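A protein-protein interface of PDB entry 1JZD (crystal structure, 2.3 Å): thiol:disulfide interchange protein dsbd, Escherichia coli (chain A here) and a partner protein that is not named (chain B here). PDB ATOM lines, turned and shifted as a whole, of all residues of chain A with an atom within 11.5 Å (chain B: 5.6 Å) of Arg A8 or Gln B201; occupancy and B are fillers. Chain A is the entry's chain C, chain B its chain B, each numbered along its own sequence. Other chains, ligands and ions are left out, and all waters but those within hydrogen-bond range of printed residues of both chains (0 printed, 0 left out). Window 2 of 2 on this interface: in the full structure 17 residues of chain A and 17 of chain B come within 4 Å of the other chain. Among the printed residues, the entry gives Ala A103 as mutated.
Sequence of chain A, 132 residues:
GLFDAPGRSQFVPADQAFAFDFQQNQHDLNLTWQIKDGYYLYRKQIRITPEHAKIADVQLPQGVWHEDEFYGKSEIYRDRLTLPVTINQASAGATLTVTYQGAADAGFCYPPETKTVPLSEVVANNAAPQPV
N of Arg A8 lies close to O of Tyr B200. The backbone carbonyl oxygen (O) of Ala A106 lies close to the backbone carbonyl oxygen (O) of Tyr B200 (3.3 Å). N of Tyr B200 lies within hydrogen-bond range of O of Gly A107 (2.8 Å).
The side-chain hydroxyl (OH) of Tyr B115 is in hydrogen-bond range of the backbone carbonyl oxygen (O) of Gln B201, 2.6 Å away. The backbone carbonyl oxygen (O) of Ala A106 is in hydrogen-bond range of the backbone NH (N) of Arg A8 (2.9 Å).
CB of Arg A8 touches O of Pro B198 (3.5 Å). Arg A8 touches Gly B199 (CB to C, 3.6 Å). CB of Arg A8 touches CG of Gln B201 (3.8 Å). O of Pro B198 touches CE1 of Phe A11, 3.7 Å away. Gly B199 touches Phe A11. Gly A107 touches Gly B199 (O to CA, 3.1 Å). Phe A108 touches Pro B198 (CE1 to CB, 3.8 Å). Phe A108 touches Gly B199 (CD1 to N, 3.8 Å).
Printed residues of chain B within 4 Å of Ala A106: Tyr B200 (3.3 Å). Printed residues of chain B within 4 Å of Gly A107: Gly B199 and Tyr B200. Of the printed residues of chain B, Phe A108 touches Pro B198 and Gly B199. No residue of chain A comes within 4 Å of Leu B108. Of the printed residues of chain A, Pro B198 touches Arg A8 (3.5 Å), Phe A11 (3.7 Å) and Phe A108 (3.8 Å). Gly B199 touches just these residues of chain A: Arg A8, Phe A11, Gly A107 and Phe A108. Tyr B200 touches just these residues of chain A: Arg A8 (3.2 Å), Ala A106 (3.3 Å) and Gly A107 (2.8 Å). Of chain A, only Arg A8 (3.8 Å) comes within 4 Å of Gln B201. No residue of chain A comes within 4 Å of Pro B202. No residue of chain A comes within 4 Å of Met B206. No residue of chain A comes within 4 Å of Phe B209. The nearest printed residue of chain B that does not touch Arg A8 is Val B197 (5.6 Å). The nearest residue of chain A that does not touch Gln B201 is Ala A106 (5.6 Å).
Hydrophobic or aromatic side chains of chain A within 4 Å of the printed part of chain B: Phe A11 and Phe A108. Of the 13 printed residues of chain B, 4 touch a printed residue of chain A. Among the printed residues, 11 pairs touch across the chains. Among the printed residues, no Asp or Glu carboxylate lies within 4 Å of a Lys or Arg side-chain nitrogen of the other chain.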
ATOM      1  N   ARG A   8     -30.033  24.352   2.075  1.00  0.00           N
ATOM      2  CA  ARG A   8     -30.188  25.782   2.473  1.00  0.00           C
ATOM      3  C   ARG A   8     -31.599  26.281   2.155  1.00  0.00           C
ATOM      4  O   ARG A   8     -31.915  26.574   1.001  1.00  0.00           O
ATOM      5  CB  ARG A   8     -29.155  26.634   1.743  1.00  0.00           C
ATOM      6  N   SER A   9     -32.436  26.386   3.188  1.00  0.00           N
ATOM      7  CA  SER A   9     -33.820  26.830   3.031  1.00  0.00           C
ATOM      8  C   SER A   9     -34.103  28.126   3.789  1.00  0.00           C
ATOM      9  O   SER A   9     -33.342  29.089   3.702  1.00  0.00           O
ATOM     10  CB  SER A   9     -34.764  25.742   3.537  1.00  0.00           C
ATOM     11  OG  SER A   9     -34.195  24.460   3.348  1.00  0.00           O
ATOM     12  N   GLN A  10     -35.209  28.131   4.533  1.00  0.00           N
ATOM     13  CA  GLN A  10     -35.634  29.287   5.324  1.00  0.00           C
ATOM     14  C   GLN A  10     -34.957  29.304   6.696  1.00  0.00           C
ATOM     15  O   GLN A  10     -35.340  28.549   7.588  1.00  0.00           O
ATOM     16  CB  GLN A  10     -37.153  29.246   5.522  1.00  0.00           C
ATOM     17  CG  GLN A  10     -37.897  30.467   4.997  1.00  0.00           C
ATOM     18  CD  GLN A  10     -37.380  31.768   5.591  1.00  0.00           C
ATOM     19  OE1 GLN A  10     -37.468  31.995   6.800  1.00  0.00           O
ATOM     20  NE2 GLN A  10     -36.835  32.628   4.737  1.00  0.00           N
ATOM     21  N   PHE A  11     -33.961  30.171   6.865  1.00  0.00           N
ATOM     22  CA  PHE A  11     -33.244  30.279   8.134  1.00  0.00           C
ATOM     23  C   PHE A  11     -33.764  31.430   8.988  1.00  0.00           C
ATOM     24  O   PHE A  11     -33.562  32.608   8.678  1.00  0.00           O
ATOM     25  CB  PHE A  11     -31.754  30.438   7.871  1.00  0.00           C
ATOM     26  CG  PHE A  11     -31.144  29.249   7.199  1.00  0.00           C
ATOM     27  CD1 PHE A  11     -30.597  29.360   5.923  1.00  0.00           C
ATOM     28  CD2 PHE A  11     -31.138  28.006   7.827  1.00  0.00           C
ATOM     29  CE1 PHE A  11     -30.049  28.252   5.279  1.00  0.00           C
ATOM     30  CE2 PHE A  11     -30.592  26.888   7.196  1.00  0.00           C
ATOM     31  CZ  PHE A  11     -30.046  27.015   5.916  1.00  0.00           C
ATOM     32  N   VAL A  12     -34.440  31.074  10.074  1.00  0.00           N
ATOM     33  CA  VAL A  12     -35.029  32.058  10.967  1.00  0.00           C
ATOM     34  C   VAL A  12     -33.997  32.733  11.858  1.00  0.00           C
ATOM     35  O   VAL A  12     -32.860  32.288  11.960  1.00  0.00           O
ATOM     36  CB  VAL A  12     -36.101  31.400  11.869  1.00  0.00           C
ATOM     37  CG1 VAL A  12     -37.138  30.649  10.996  1.00  0.00           C
ATOM     38  CG2 VAL A  12     -35.433  30.449  12.872  1.00  0.00           C
ATOM     39  N   GLY A  38     -34.465  21.178  13.001  1.00  0.00           N
ATOM     40  CA  GLY A  38     -33.542  21.489  11.924  1.00  0.00           C
ATOM     41  C   GLY A  38     -32.373  22.363  12.374  1.00  0.00           C
ATOM     42  O   GLY A  38     -31.561  22.820  11.545  1.00  0.00           O
ATOM     43  N   TYR A  39     -32.282  22.583  13.689  1.00  0.00           N
ATOM     44  CA  TYR A  39     -31.222  23.397  14.281  1.00  0.00           C
ATOM     45  C   TYR A  39     -30.606  22.675  15.471  1.00  0.00           C
ATOM     46  O   TYR A  39     -31.199  21.755  16.016  1.00  0.00           O
ATOM     47  CB  TYR A  39     -31.788  24.741  14.735  1.00  0.00           C
ATOM     48  CG  TYR A  39     -32.386  25.559  13.610  1.00  0.00           C
ATOM     49  CD1 TYR A  39     -33.600  25.205  13.022  1.00  0.00           C
ATOM     50  CD2 TYR A  39     -31.731  26.681  13.132  1.00  0.00           C
ATOM     51  CE1 TYR A  39     -34.143  25.965  11.980  1.00  0.00           C
ATOM     52  CE2 TYR A  39     -32.253  27.438  12.101  1.00  0.00           C
ATOM     53  CZ  TYR A  39     -33.455  27.083  11.526  1.00  0.00           C
ATOM     54  OH  TYR A  39     -33.946  27.861  10.502  1.00  0.00           O
ATOM     55  N   ALA A 103     -26.249  26.071  14.886  1.00  0.00           N
ATOM     56  CA  ALA A 103     -26.225  26.020  13.440  1.00  0.00           C
ATOM     57  C   ALA A 103     -27.483  25.332  12.932  1.00  0.00           C
ATOM     58  O   ALA A 103     -28.327  24.926  13.727  1.00  0.00           O
ATOM     59  CB  ALA A 103     -24.981  25.265  12.997  1.00  0.00           C
ATOM     60  N   ALA A 104     -27.607  25.208  11.612  1.00  0.00           N
ATOM     61  CA  ALA A 104     -28.772  24.558  11.012  1.00  0.00           C
ATOM     62  C   ALA A 104     -28.363  23.479  10.006  1.00  0.00           C
ATOM     63  O   ALA A 104     -27.469  23.686   9.185  1.00  0.00           O
ATOM     64  CB  ALA A 104     -29.656  25.592  10.342  1.00  0.00           C
ATOM     65  N   ASP A 105     -29.028  22.327  10.097  1.00  0.00           N
ATOM     66  CA  ASP A 105     -28.787  21.165   9.233  1.00  0.00           C
ATOM     67  C   ASP A 105     -28.715  21.535   7.759  1.00  0.00           C
ATOM     68  O   ASP A 105     -27.905  20.996   7.007  1.00  0.00           O
ATOM     69  CB  ASP A 105     -29.914  20.136   9.400  1.00  0.00           C
ATOM     70  CG  ASP A 105     -29.948  19.504  10.776  1.00  0.00           C
ATOM     71  OD1 ASP A 105     -31.067  19.210  11.256  1.00  0.00           O
ATOM     72  OD2 ASP A 105     -28.877  19.280  11.370  1.00  0.00           O
ATOM     73  N   ALA A 106     -29.587  22.441   7.351  1.00  0.00           N
ATOM     74  CA  ALA A 106     -29.646  22.873   5.963  1.00  0.00           C
ATOM     75  C   ALA A 106     -28.380  23.589   5.494  1.00  0.00           C
ATOM     76  O   ALA A 106     -28.349  24.111   4.382  1.00  0.00           O
ATOM     77  CB  ALA A 106     -30.868  23.763   5.747  1.00  0.00           C
ATOM     78  N   GLY A 107     -27.355  23.625   6.345  1.00  0.00           N
ATOM     79  CA  GLY A 107     -26.089  24.239   5.974  1.00  0.00           C
ATOM     80  C   GLY A 107     -25.913  25.703   6.313  1.00  0.00           C
ATOM     81  O   GLY A 107     -25.726  26.533   5.428  1.00  0.00           O
ATOM     82  N   PHE A 108     -25.930  26.024   7.600  1.00  0.00           N
ATOM     83  CA  PHE A 108     -25.811  27.413   8.014  1.00  0.00           C
ATOM     84  C   PHE A 108     -25.270  27.498   9.431  1.00  0.00           C
ATOM     85  O   PHE A 108     -25.732  26.770  10.313  1.00  0.00           O
ATOM     86  CB  PHE A 108     -27.202  28.049   7.948  1.00  0.00           C
ATOM     87  CG  PHE A 108     -27.204  29.544   7.999  1.00  0.00           C
ATOM     88  CD1 PHE A 108     -26.538  30.292   7.030  1.00  0.00           C
ATOM     89  CD2 PHE A 108     -27.944  30.212   8.970  1.00  0.00           C
ATOM     90  CE1 PHE A 108     -26.615  31.688   7.021  1.00  0.00           C
ATOM     91  CE2 PHE A 108     -28.027  31.607   8.973  1.00  0.00           C
ATOM     92  CZ  PHE A 108     -27.363  32.348   7.991  1.00  0.00           C
ATOM     93  N   CYS A 109     -24.269  28.351   9.641  1.00  0.00           N
ATOM     94  CA  CYS A 109     -23.722  28.556  10.983  1.00  0.00           C
ATOM     95  C   CYS A 109     -24.051  29.966  11.400  1.00  0.00           C
ATOM     96  O   CYS A 109     -23.856  30.917  10.645  1.00  0.00           O
ATOM     97  CB  CYS A 109     -22.206  28.408  11.050  1.00  0.00           C
ATOM     98  SG  CYS A 109     -21.533  26.834  10.465  1.00  0.00           S
ATOM     99  N   TYR A 110     -24.552  30.097  12.613  1.00  0.00           N
ATOM    100  CA  TYR A 110     -24.905  31.395  13.149  1.00  0.00           C
ATOM    101  C   TYR A 110     -23.750  31.940  13.965  1.00  0.00           C
ATOM    102  O   TYR A 110     -22.871  31.195  14.393  1.00  0.00           O
ATOM    103  CB  TYR A 110     -26.095  31.289  14.088  1.00  0.00           C
ATOM    104  CG  TYR A 110     -27.413  31.032  13.430  1.00  0.00           C
ATOM    105  CD1 TYR A 110     -27.808  29.739  13.076  1.00  0.00           C
ATOM    106  CD2 TYR A 110     -28.286  32.084  13.178  1.00  0.00           C
ATOM    107  CE1 TYR A 110     -29.044  29.509  12.493  1.00  0.00           C
ATOM    108  CE2 TYR A 110     -29.520  31.864  12.595  1.00  0.00           C
ATOM    109  CZ  TYR A 110     -29.896  30.582  12.252  1.00  0.00           C
ATOM    110  OH  TYR A 110     -31.123  30.392  11.656  1.00  0.00           O
ATOM    111  N   LEU B 108     -18.624  23.034   1.789  1.00  0.00           N
ATOM    112  CA  LEU B 108     -18.771  23.643   0.478  1.00  0.00           C
ATOM    113  C   LEU B 108     -17.449  23.610  -0.281  1.00  0.00           C
ATOM    114  O   LEU B 108     -17.404  23.177  -1.429  1.00  0.00           O
ATOM    115  CB  LEU B 108     -19.266  25.084   0.618  1.00  0.00           C
ATOM    116  CG  LEU B 108     -19.697  25.815  -0.655  1.00  0.00           C
ATOM    117  CD1 LEU B 108     -20.520  27.039  -0.283  1.00  0.00           C
ATOM    118  CD2 LEU B 108     -18.484  26.229  -1.458  1.00  0.00           C
ATOM    119  N   TYR B 115     -18.434  21.849  -7.997  1.00  0.00           N
ATOM    120  CA  TYR B 115     -19.164  23.060  -8.387  1.00  0.00           C
ATOM    121  C   TYR B 115     -18.583  23.488  -9.731  1.00  0.00           C
ATOM    122  O   TYR B 115     -19.313  23.794 -10.669  1.00  0.00           O
ATOM    123  CB  TYR B 115     -18.956  24.195  -7.371  1.00  0.00           C
ATOM    124  CG  TYR B 115     -19.653  23.985  -6.050  1.00  0.00           C
ATOM    125  CD1 TYR B 115     -21.037  24.150  -5.934  1.00  0.00           C
ATOM    126  CD2 TYR B 115     -18.935  23.583  -4.918  1.00  0.00           C
ATOM    127  CE1 TYR B 115     -21.689  23.917  -4.721  1.00  0.00           C
ATOM    128  CE2 TYR B 115     -19.574  23.343  -3.703  1.00  0.00           C
ATOM    129  CZ  TYR B 115     -20.945  23.511  -3.610  1.00  0.00           C
ATOM    130  OH  TYR B 115     -21.572  23.273  -2.411  1.00  0.00           O
ATOM    131  N   VAL B 189     -24.506  32.996  -0.037  1.00  0.00           N
ATOM    132  CA  VAL B 189     -24.271  33.152  -1.460  1.00  0.00           C
ATOM    133  C   VAL B 189     -24.877  34.415  -2.030  1.00  0.00           C
ATOM    134  O   VAL B 189     -26.006  34.749  -1.725  1.00  0.00           O
ATOM    135  CB  VAL B 189     -24.831  31.949  -2.250  1.00  0.00           C
ATOM    136  CG1 VAL B 189     -24.495  32.112  -3.732  1.00  0.00           C
ATOM    137  CG2 VAL B 189     -24.262  30.634  -1.693  1.00  0.00           C
ATOM    138  N   VAL B 197     -28.609  34.552  -0.955  1.00  0.00           N
ATOM    139  CA  VAL B 197     -29.135  33.217  -0.713  1.00  0.00           C
ATOM    140  C   VAL B 197     -28.283  32.576   0.375  1.00  0.00           C
ATOM    141  O   VAL B 197     -27.290  31.908   0.091  1.00  0.00           O
ATOM    142  CB  VAL B 197     -29.069  32.328  -1.980  1.00  0.00           C
ATOM    143  CG1 VAL B 197     -29.717  30.982  -1.706  1.00  0.00           C
ATOM    144  CG2 VAL B 197     -29.756  33.025  -3.146  1.00  0.00           C
ATOM    145  N   PRO B 198     -28.664  32.779   1.641  1.00  0.00           N
ATOM    146  CA  PRO B 198     -27.935  32.222   2.783  1.00  0.00           C
ATOM    147  C   PRO B 198     -27.877  30.701   2.787  1.00  0.00           C
ATOM    148  O   PRO B 198     -28.806  30.034   2.345  1.00  0.00           O
ATOM    149  CB  PRO B 198     -28.719  32.750   3.985  1.00  0.00           C
ATOM    150  CG  PRO B 198     -29.352  34.007   3.469  1.00  0.00           C
ATOM    151  CD  PRO B 198     -29.798  33.601   2.093  1.00  0.00           C
ATOM    152  N   GLY B 199     -26.769  30.160   3.284  1.00  0.00           N
ATOM    153  CA  GLY B 199     -26.634  28.720   3.385  1.00  0.00           C
ATOM    154  C   GLY B 199     -25.889  27.974   2.298  1.00  0.00           C
ATOM    155  O   GLY B 199     -25.677  28.472   1.195  1.00  0.00           O
ATOM    156  N   TYR B 200     -25.503  26.751   2.639  1.00  0.00           N
ATOM    157  CA  TYR B 200     -24.785  25.839   1.760  1.00  0.00           C
ATOM    158  C   TYR B 200     -25.750  24.959   0.964  1.00  0.00           C
ATOM    159  O   TYR B 200     -26.791  24.540   1.472  1.00  0.00           O
ATOM    160  CB  TYR B 200     -23.877  24.930   2.597  1.00  0.00           C
ATOM    161  CG  TYR B 200     -23.624  23.562   1.994  1.00  0.00           C
ATOM    162  CD1 TYR B 200     -22.597  23.360   1.068  1.00  0.00           C
ATOM    163  CD2 TYR B 200     -24.428  22.465   2.339  1.00  0.00           C
ATOM    164  CE1 TYR B 200     -22.370  22.108   0.501  1.00  0.00           C
ATOM    165  CE2 TYR B 200     -24.213  21.206   1.774  1.00  0.00           C
ATOM    166  CZ  TYR B 200     -23.181  21.034   0.855  1.00  0.00           C
ATOM    167  OH  TYR B 200     -22.972  19.800   0.273  1.00  0.00           O
ATOM    168  N   GLN B 201     -25.384  24.675  -0.281  1.00  0.00           N
ATOM    169  CA  GLN B 201     -26.177  23.807  -1.147  1.00  0.00           C
ATOM    170  C   GLN B 201     -25.203  22.881  -1.862  1.00  0.00           C
ATOM    171  O   GLN B 201     -24.151  23.323  -2.345  1.00  0.00           O
ATOM    172  CB  GLN B 201     -26.931  24.616  -2.194  1.00  0.00           C
ATOM    173  CG  GLN B 201     -27.911  25.621  -1.647  1.00  0.00           C
ATOM    174  CD  GLN B 201     -28.668  26.300  -2.766  1.00  0.00           C
ATOM    175  OE1 GLN B 201     -29.368  25.646  -3.546  1.00  0.00           O
ATOM    176  NE2 GLN B 201     -28.526  27.613  -2.865  1.00  0.00           N
ATOM    177  N   PRO B 202     -25.520  21.580  -1.921  1.00  0.00           N
ATOM    178  CA  PRO B 202     -24.607  20.660  -2.609  1.00  0.00           C
ATOM    179  C   PRO B 202     -24.501  21.071  -4.085  1.00  0.00           C
ATOM    180  O   PRO B 202     -25.372  21.779  -4.607  1.00  0.00           O
ATOM    181  CB  PRO B 202     -25.282  19.295  -2.433  1.00  0.00           C
ATOM    182  CG  PRO B 202     -26.087  19.451  -1.166  1.00  0.00           C
ATOM    183  CD  PRO B 202     -26.647  20.857  -1.300  1.00  0.00           C
ATOM    184  N   PRO B 203     -23.427  20.646  -4.773  1.00  0.00           N
ATOM    185  CA  PRO B 203     -23.240  20.988  -6.187  1.00  0.00           C
ATOM    186  C   PRO B 203     -24.503  20.819  -7.035  1.00  0.00           C
ATOM    187  O   PRO B 203     -25.013  21.788  -7.592  1.00  0.00           O
ATOM    188  CB  PRO B 203     -22.113  20.056  -6.607  1.00  0.00           C
ATOM    189  CG  PRO B 203     -21.263  20.019  -5.366  1.00  0.00           C
ATOM    190  CD  PRO B 203     -22.305  19.819  -4.287  1.00  0.00           C
ATOM    191  N   GLU B 205     -27.735  20.440  -6.333  1.00  0.00           N
ATOM    192  CA  GLU B 205     -28.847  21.311  -5.968  1.00  0.00           C
ATOM    193  C   GLU B 205     -28.546  22.770  -6.284  1.00  0.00           C
ATOM    194  O   GLU B 205     -29.430  23.520  -6.702  1.00  0.00           O
ATOM    195  CB  GLU B 205     -29.202  21.138  -4.490  1.00  0.00           C
ATOM    196  CG  GLU B 205     -29.898  19.808  -4.182  1.00  0.00           C
ATOM    197  CD  GLU B 205     -28.936  18.621  -4.048  1.00  0.00           C
ATOM    198  OE1 GLU B 205     -27.986  18.502  -4.857  1.00  0.00           O
ATOM    199  OE2 GLU B 205     -29.139  17.790  -3.131  1.00  0.00           O
ATOM    200  N   MET B 206     -27.296  23.174  -6.089  1.00  0.00           N
ATOM    201  CA  MET B 206     -26.892  24.543  -6.400  1.00  0.00           C
ATOM    202  C   MET B 206     -27.017  24.756  -7.914  1.00  0.00           C
ATOM    203  O   MET B 206     -27.600  25.744  -8.375  1.00  0.00           O
ATOM    204  CB  MET B 206     -25.438  24.775  -5.981  1.00  0.00           C
ATOM    205  CG  MET B 206     -24.901  26.157  -6.301  1.00  0.00           C
ATOM    206  SD  MET B 206     -25.513  27.422  -5.173  1.00  0.00           S
ATOM    207  CE  MET B 206     -24.527  27.021  -3.695  1.00  0.00           C
ATOM    208  N   PHE B 209     -30.559  24.953  -8.784  1.00  0.00           N
ATOM    209  CA  PHE B 209     -31.152  26.186  -8.283  1.00  0.00           C
ATOM    210  C   PHE B 209     -30.707  27.371  -9.133  1.00  0.00           C
ATOM    211  O   PHE B 209     -31.495  28.266  -9.428  1.00  0.00           O
ATOM    212  CB  PHE B 209     -30.754  26.447  -6.823  1.00  0.00           C
ATOM    213  CG  PHE B 209     -31.109  27.829  -6.350  1.00  0.00           C
ATOM    214  CD1 PHE B 209     -32.410  28.134  -5.963  1.00  0.00           C
ATOM    215  CD2 PHE B 209     -30.156  28.845  -6.359  1.00  0.00           C
ATOM    216  CE1 PHE B 209     -32.761  29.429  -5.591  1.00  0.00           C
ATOM    217  CE2 PHE B 209     -30.492  30.147  -5.992  1.00  0.00           C
ATOM    218  CZ  PHE B 209     -31.799  30.439  -5.607  1.00  0.00           C
